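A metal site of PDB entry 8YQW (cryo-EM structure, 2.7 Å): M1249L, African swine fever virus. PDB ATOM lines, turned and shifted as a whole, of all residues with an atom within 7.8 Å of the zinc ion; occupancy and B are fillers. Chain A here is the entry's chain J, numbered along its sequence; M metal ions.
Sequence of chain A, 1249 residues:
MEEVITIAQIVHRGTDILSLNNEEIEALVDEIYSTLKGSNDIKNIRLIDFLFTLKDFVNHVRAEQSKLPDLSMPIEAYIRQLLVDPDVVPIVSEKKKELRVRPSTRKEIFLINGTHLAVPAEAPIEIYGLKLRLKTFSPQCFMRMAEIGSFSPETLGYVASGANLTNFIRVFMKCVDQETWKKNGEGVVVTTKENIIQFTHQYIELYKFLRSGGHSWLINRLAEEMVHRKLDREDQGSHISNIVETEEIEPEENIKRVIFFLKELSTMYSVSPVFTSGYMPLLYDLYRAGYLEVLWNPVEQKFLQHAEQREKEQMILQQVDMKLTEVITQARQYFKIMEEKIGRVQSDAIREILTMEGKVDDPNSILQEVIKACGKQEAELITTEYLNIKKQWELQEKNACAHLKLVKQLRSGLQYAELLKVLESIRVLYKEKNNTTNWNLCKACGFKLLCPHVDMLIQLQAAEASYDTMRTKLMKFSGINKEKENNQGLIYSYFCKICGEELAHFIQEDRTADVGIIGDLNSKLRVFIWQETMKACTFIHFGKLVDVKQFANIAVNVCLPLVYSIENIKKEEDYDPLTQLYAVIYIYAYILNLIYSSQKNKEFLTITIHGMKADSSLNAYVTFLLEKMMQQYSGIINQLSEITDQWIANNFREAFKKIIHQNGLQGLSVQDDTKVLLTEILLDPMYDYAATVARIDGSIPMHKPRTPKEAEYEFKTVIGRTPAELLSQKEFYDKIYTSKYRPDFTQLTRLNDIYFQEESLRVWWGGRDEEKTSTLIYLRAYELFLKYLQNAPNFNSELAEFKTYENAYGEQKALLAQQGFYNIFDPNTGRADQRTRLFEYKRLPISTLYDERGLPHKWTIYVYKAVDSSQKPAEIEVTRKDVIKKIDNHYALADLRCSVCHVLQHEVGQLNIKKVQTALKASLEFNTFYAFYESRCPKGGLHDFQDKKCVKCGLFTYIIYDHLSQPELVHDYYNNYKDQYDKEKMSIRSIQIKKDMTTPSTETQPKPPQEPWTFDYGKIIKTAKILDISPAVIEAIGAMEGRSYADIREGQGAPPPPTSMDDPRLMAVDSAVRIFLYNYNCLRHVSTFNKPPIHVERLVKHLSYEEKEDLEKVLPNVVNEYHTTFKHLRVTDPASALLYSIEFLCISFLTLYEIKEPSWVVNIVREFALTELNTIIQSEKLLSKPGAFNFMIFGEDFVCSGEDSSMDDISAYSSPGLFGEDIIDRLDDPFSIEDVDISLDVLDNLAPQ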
ATOM      1  N   SER A 847       8.084  15.533 -12.882  1.00  0.00           N
ATOM      2  CA  SER A 847       7.471  14.229 -12.686  1.00  0.00           C
ATOM      3  C   SER A 847       7.964  13.193 -13.690  1.00  0.00           C
ATOM      4  O   SER A 847       7.765  12.001 -13.467  1.00  0.00           O
ATOM      5  CB  SER A 847       5.949  14.347 -12.782  1.00  0.00           C
ATOM      6  OG  SER A 847       5.542  14.721 -14.087  1.00  0.00           O
ATOM      7  N   LEU A 849      10.979  12.457 -14.077  1.00  0.00           N
ATOM      8  CA  LEU A 849      12.154  11.862 -13.466  1.00  0.00           C
ATOM      9  C   LEU A 849      11.909  11.321 -12.072  1.00  0.00           C
ATOM     10  O   LEU A 849      12.614  10.391 -11.651  1.00  0.00           O
ATOM     11  CB  LEU A 849      13.294  12.883 -13.396  1.00  0.00           C
ATOM     12  CG  LEU A 849      13.939  13.350 -14.697  1.00  0.00           C
ATOM     13  CD1 LEU A 849      14.968  14.422 -14.406  1.00  0.00           C
ATOM     14  CD2 LEU A 849      14.582  12.187 -15.425  1.00  0.00           C
ATOM     15  N   TYR A 850      10.940  11.854 -11.329  1.00  0.00           N
ATOM     16  CA  TYR A 850      10.698  11.461  -9.952  1.00  0.00           C
ATOM     17  C   TYR A 850       9.206  11.265  -9.716  1.00  0.00           C
ATOM     18  O   TYR A 850       8.365  11.847 -10.406  1.00  0.00           O
ATOM     19  CB  TYR A 850      11.245  12.519  -8.983  1.00  0.00           C
ATOM     20  CG  TYR A 850      12.722  12.776  -9.136  1.00  0.00           C
ATOM     21  CD1 TYR A 850      13.648  11.971  -8.497  1.00  0.00           C
ATOM     22  CD2 TYR A 850      13.186  13.794  -9.933  1.00  0.00           C
ATOM     23  CE1 TYR A 850      15.003  12.190  -8.646  1.00  0.00           C
ATOM     24  CE2 TYR A 850      14.538  14.027 -10.080  1.00  0.00           C
ATOM     25  CZ  TYR A 850      15.440  13.217  -9.439  1.00  0.00           C
ATOM     26  OH  TYR A 850      16.789  13.443  -9.592  1.00  0.00           O
ATOM     27  N   ASP A 851       8.887  10.429  -8.733  1.00  0.00           N
ATOM     28  CA  ASP A 851       7.507  10.098  -8.422  1.00  0.00           C
ATOM     29  C   ASP A 851       7.005  10.986  -7.284  1.00  0.00           C
ATOM     30  O   ASP A 851       7.723  11.850  -6.770  1.00  0.00           O
ATOM     31  CB  ASP A 851       7.373   8.618  -8.097  1.00  0.00           C
ATOM     32  CG  ASP A 851       8.255   8.185  -6.933  1.00  0.00           C
ATOM     33  OD1 ASP A 851       9.055   9.013  -6.449  1.00  0.00           O
ATOM     34  OD2 ASP A 851       8.147   7.029  -6.502  1.00  0.00           O
ATOM     35  N   GLU A 852       5.761  10.763  -6.857  1.00  0.00           N
ATOM     36  CA  GLU A 852       5.158  11.570  -5.801  1.00  0.00           C
ATOM     37  C   GLU A 852       5.785  11.316  -4.436  1.00  0.00           C
ATOM     38  O   GLU A 852       5.474  12.059  -3.494  1.00  0.00           O
ATOM     39  CB  GLU A 852       3.649  11.302  -5.750  1.00  0.00           C
ATOM     40  CG  GLU A 852       2.894  11.858  -6.942  1.00  0.00           C
ATOM     41  CD  GLU A 852       1.462  11.364  -6.999  1.00  0.00           C
ATOM     42  OE1 GLU A 852       1.125  10.405  -6.270  1.00  0.00           O
ATOM     43  OE2 GLU A 852       0.671  11.931  -7.778  1.00  0.00           O
ATOM     44  N   LEU A 855      11.229   9.561  -5.323  1.00  0.00           N
ATOM     45  CA  LEU A 855      12.255   8.653  -5.789  1.00  0.00           C
ATOM     46  C   LEU A 855      12.367   8.685  -7.309  1.00  0.00           C
ATOM     47  O   LEU A 855      11.379   8.940  -8.009  1.00  0.00           O
ATOM     48  CB  LEU A 855      11.958   7.236  -5.329  1.00  0.00           C
ATOM     49  CG  LEU A 855      11.453   7.088  -3.890  1.00  0.00           C
ATOM     50  CD1 LEU A 855      11.143   5.638  -3.565  1.00  0.00           C
ATOM     51  CD2 LEU A 855      12.455   7.654  -2.908  1.00  0.00           C
ATOM     52  N   PRO A 856      13.552   8.425  -7.862  1.00  0.00           N
ATOM     53  CA  PRO A 856      13.692   8.421  -9.318  1.00  0.00           C
ATOM     54  C   PRO A 856      13.009   7.221  -9.951  1.00  0.00           C
ATOM     55  O   PRO A 856      12.783   6.183  -9.328  1.00  0.00           O
ATOM     56  CB  PRO A 856      15.216   8.351  -9.527  1.00  0.00           C
ATOM     57  CG  PRO A 856      15.744   7.778  -8.270  1.00  0.00           C
ATOM     58  CD  PRO A 856      14.839   8.236  -7.173  1.00  0.00           C
ATOM     59  N   HIS A 857      12.651   7.383 -11.220  1.00  0.00           N
ATOM     60  CA  HIS A 857      12.038   6.309 -11.990  1.00  0.00           C
ATOM     61  C   HIS A 857      13.104   5.349 -12.494  1.00  0.00           C
ATOM     62  O   HIS A 857      14.231   5.738 -12.818  1.00  0.00           O
ATOM     63  CB  HIS A 857      11.249   6.870 -13.172  1.00  0.00           C
ATOM     64  CG  HIS A 857       9.992   7.577 -12.778  1.00  0.00           C
ATOM     65  ND1 HIS A 857       9.058   7.038 -11.923  1.00  0.00           N
ATOM     66  CD2 HIS A 857       9.517   8.790 -13.143  1.00  0.00           C
ATOM     67  CE1 HIS A 857       8.063   7.892 -11.768  1.00  0.00           C
ATOM     68  NE2 HIS A 857       8.313   8.961 -12.491  1.00  0.00           N
ATOM     69  N   LYS A 858      12.733   4.060 -12.563  1.00  0.00           N
ATOM     70  CA  LYS A 858      13.599   3.010 -13.092  1.00  0.00           C
ATOM     71  C   LYS A 858      12.762   2.192 -14.078  1.00  0.00           C
ATOM     72  O   LYS A 858      12.101   1.230 -13.697  1.00  0.00           O
ATOM     73  CB  LYS A 858      14.168   2.155 -11.973  1.00  0.00           C
ATOM     74  CG  LYS A 858      15.195   2.873 -11.122  1.00  0.00           C
ATOM     75  CD  LYS A 858      15.868   1.926 -10.140  1.00  0.00           C
ATOM     76  CE  LYS A 858      16.918   2.660  -9.319  1.00  0.00           C
ATOM     77  NZ  LYS A 858      16.305   3.696  -8.435  1.00  0.00           N
ATOM     78  N   TRP A 859      12.811   2.584 -15.346  1.00  0.00           N
ATOM     79  CA  TRP A 859      11.993   1.958 -16.376  1.00  0.00           C
ATOM     80  C   TRP A 859      12.538   0.594 -16.749  1.00  0.00           C
ATOM     81  O   TRP A 859      13.306   0.476 -17.715  1.00  0.00           O
ATOM     82  CB  TRP A 859      11.904   2.861 -17.604  1.00  0.00           C
ATOM     83  CG  TRP A 859      11.472   4.249 -17.266  1.00  0.00           C
ATOM     84  CD1 TRP A 859      12.224   5.382 -17.340  1.00  0.00           C
ATOM     85  CD2 TRP A 859      10.185   4.653 -16.789  1.00  0.00           C
ATOM     86  NE1 TRP A 859      11.489   6.464 -16.946  1.00  0.00           N
ATOM     87  CE2 TRP A 859      10.232   6.048 -16.592  1.00  0.00           C
ATOM     88  CE3 TRP A 859       9.000   3.977 -16.499  1.00  0.00           C
ATOM     89  CZ2 TRP A 859       9.134   6.765 -16.140  1.00  0.00           C
ATOM     90  CZ3 TRP A 859       7.918   4.697 -16.043  1.00  0.00           C
ATOM     91  CH2 TRP A 859       7.988   6.078 -15.873  1.00  0.00           C
ATOM     92  N   ARG A 897       7.561   0.207 -17.717  1.00  0.00           N
ATOM     93  CA  ARG A 897       7.039   0.410 -16.381  1.00  0.00           C
ATOM     94  C   ARG A 897       8.184   0.624 -15.404  1.00  0.00           C
ATOM     95  O   ARG A 897       9.255   0.028 -15.546  1.00  0.00           O
ATOM     96  CB  ARG A 897       6.163  -0.765 -15.934  1.00  0.00           C
ATOM     97  CG  ARG A 897       5.317  -0.474 -14.712  1.00  0.00           C
ATOM     98  CD  ARG A 897       4.421  -1.652 -14.351  1.00  0.00           C
ATOM     99  NE  ARG A 897       3.252  -1.744 -15.216  1.00  0.00           N
ATOM    100  CZ  ARG A 897       2.082  -1.194 -14.938  1.00  0.00           C
ATOM    101  NH1 ARG A 897       1.876  -0.502 -13.838  1.00  0.00           N
ATOM    102  NH2 ARG A 897       1.080  -1.348 -15.810  1.00  0.00           N
ATOM    103  N   CYS A 898       7.943   1.490 -14.431  1.00  0.00           N
ATOM    104  CA  CYS A 898       8.882   1.717 -13.353  1.00  0.00           C
ATOM    105  C   CYS A 898       8.791   0.595 -12.333  1.00  0.00           C
ATOM    106  O   CYS A 898       7.712   0.084 -12.048  1.00  0.00           O
ATOM    107  CB  CYS A 898       8.631   3.061 -12.690  1.00  0.00           C
ATOM    108  SG  CYS A 898       9.836   3.528 -11.425  1.00  0.00           S
ATOM    109  N   SER A 899       9.939   0.219 -11.778  1.00  0.00           N
ATOM    110  CA  SER A 899      10.007  -0.833 -10.770  1.00  0.00           C
ATOM    111  C   SER A 899       9.909  -0.303  -9.345  1.00  0.00           C
ATOM    112  O   SER A 899      10.075  -1.062  -8.394  1.00  0.00           O
ATOM    113  CB  SER A 899      11.299  -1.629 -10.942  1.00  0.00           C
ATOM    114  OG  SER A 899      12.436  -0.794 -10.776  1.00  0.00           O
ATOM    115  N   VAL A 900       9.644   0.997  -9.179  1.00  0.00           N
ATOM    116  CA  VAL A 900       9.582   1.598  -7.858  1.00  0.00           C
ATOM    117  C   VAL A 900       8.159   2.056  -7.559  1.00  0.00           C
ATOM    118  O   VAL A 900       7.541   1.580  -6.588  1.00  0.00           O
ATOM    119  CB  VAL A 900      10.567   2.782  -7.745  1.00  0.00           C
ATOM    120  CG1 VAL A 900      10.408   3.475  -6.405  1.00  0.00           C
ATOM    121  CG2 VAL A 900      11.997   2.291  -7.925  1.00  0.00           C
ATOM    122  N   CYS A 901       7.626   2.966  -8.368  1.00  0.00           N
ATOM    123  CA  CYS A 901       6.282   3.470  -8.179  1.00  0.00           C
ATOM    124  C   CYS A 901       5.242   2.715  -8.997  1.00  0.00           C
ATOM    125  O   CYS A 901       4.040   2.920  -8.779  1.00  0.00           O
ATOM    126  CB  CYS A 901       6.208   4.961  -8.532  1.00  0.00           C
ATOM    127  SG  CYS A 901       6.659   5.337 -10.238  1.00  0.00           S
ATOM    128  N   HIS A 902       5.680   1.861  -9.915  1.00  0.00           N
ATOM    129  CA  HIS A 902       4.797   0.995 -10.708  1.00  0.00           C
ATOM    130  C   HIS A 902       3.790   1.827 -11.504  1.00  0.00           C
ATOM    131  O   HIS A 902       2.572   1.646 -11.403  1.00  0.00           O
ATOM    132  CB  HIS A 902       4.095  -0.018  -9.819  1.00  0.00           C
ATOM    133  CG  HIS A 902       5.034  -0.945  -9.104  1.00  0.00           C
ATOM    134  ND1 HIS A 902       5.656  -2.000  -9.722  1.00  0.00           N
ATOM    135  CD2 HIS A 902       5.476  -0.949  -7.820  1.00  0.00           C
ATOM    136  CE1 HIS A 902       6.432  -2.631  -8.859  1.00  0.00           C
ATOM    137  NE2 HIS A 902       6.333  -2.007  -7.695  1.00  0.00           N
ATOM    138  N   VAL A 903       4.323   2.732 -12.313  1.00  0.00           N
ATOM    139  CA  VAL A 903       3.515   3.557 -13.214  1.00  0.00           C
ATOM    140  C   VAL A 903       3.995   3.325 -14.640  1.00  0.00           C
ATOM    141  O   VAL A 903       5.183   3.073 -14.861  1.00  0.00           O
ATOM    142  CB  VAL A 903       3.580   5.053 -12.836  1.00  0.00           C
ATOM    143  CG1 VAL A 903       4.890   5.675 -13.285  1.00  0.00           C
ATOM    144  CG2 VAL A 903       2.401   5.806 -13.421  1.00  0.00           C
ATOM    145  N   VAL A 908       2.845   8.887 -16.928  1.00  0.00           N
ATOM    146  CA  VAL A 908       3.623   9.594 -15.926  1.00  0.00           C
ATOM    147  C   VAL A 908       3.093  11.007 -15.703  1.00  0.00           C
ATOM    148  O   VAL A 908       3.302  11.584 -14.631  1.00  0.00           O
ATOM    149  CB  VAL A 908       5.116   9.632 -16.315  1.00  0.00           C
ATOM    150  CG1 VAL A 908       5.339  10.527 -17.521  1.00  0.00           C
ATOM    151  CG2 VAL A 908       5.977  10.055 -15.143  1.00  0.00           C
ATOM    152  N   LEU A 911       0.801  12.062 -12.557  1.00  0.00           N
ATOM    153  CA  LEU A 911       1.337  12.339 -11.231  1.00  0.00           C
ATOM    154  C   LEU A 911       1.209  13.817 -10.920  1.00  0.00           C
ATOM    155  O   LEU A 911       1.455  14.673 -11.776  1.00  0.00           O
ATOM    156  CB  LEU A 911       2.800  11.915 -11.147  1.00  0.00           C
ATOM    157  CG  LEU A 911       3.131  10.432 -11.371  1.00  0.00           C
ATOM    158  CD1 LEU A 911       4.636  10.217 -11.362  1.00  0.00           C
ATOM    159  CD2 LEU A 911       2.460   9.556 -10.334  1.00  0.00           C
HETATM  160 ZN    ZN M   1       8.950   5.362 -10.357  1.00  0.00          ZN
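The backbone NH of His 857 is in hydrogen-bond range of the backbone carbonyl oxygen of Leu 849, at 3.0 Å. O of Val 903 sits at hydrogen-bond distance from N of Cys 898, 3.2 Å away. The backbone NH (N) of Val 900 sits close to the side-chain sulfur (SG) of Cys 898 (3.4 Å). O of Ser 847 sits at hydrogen-bond distance from NE2 of His 857 (3.2 Å). SG of Cys 898 sits close to N of Lys 858 (3.2 Å).
Of the 19 residues printed, 3 come within 4 Å of the zinc ion. The nearest printed residue that does not touch the zinc ion is Val 900 (4.01 Å).
The zinc ion is bound by the side-chain sulfur (SG) of Cys 901 (2.3 Å), a ring nitrogen (ND1) of His 857 (2.3 Å) and the side-chain sulfur (SG) of Cys 898 (2.3 Å).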
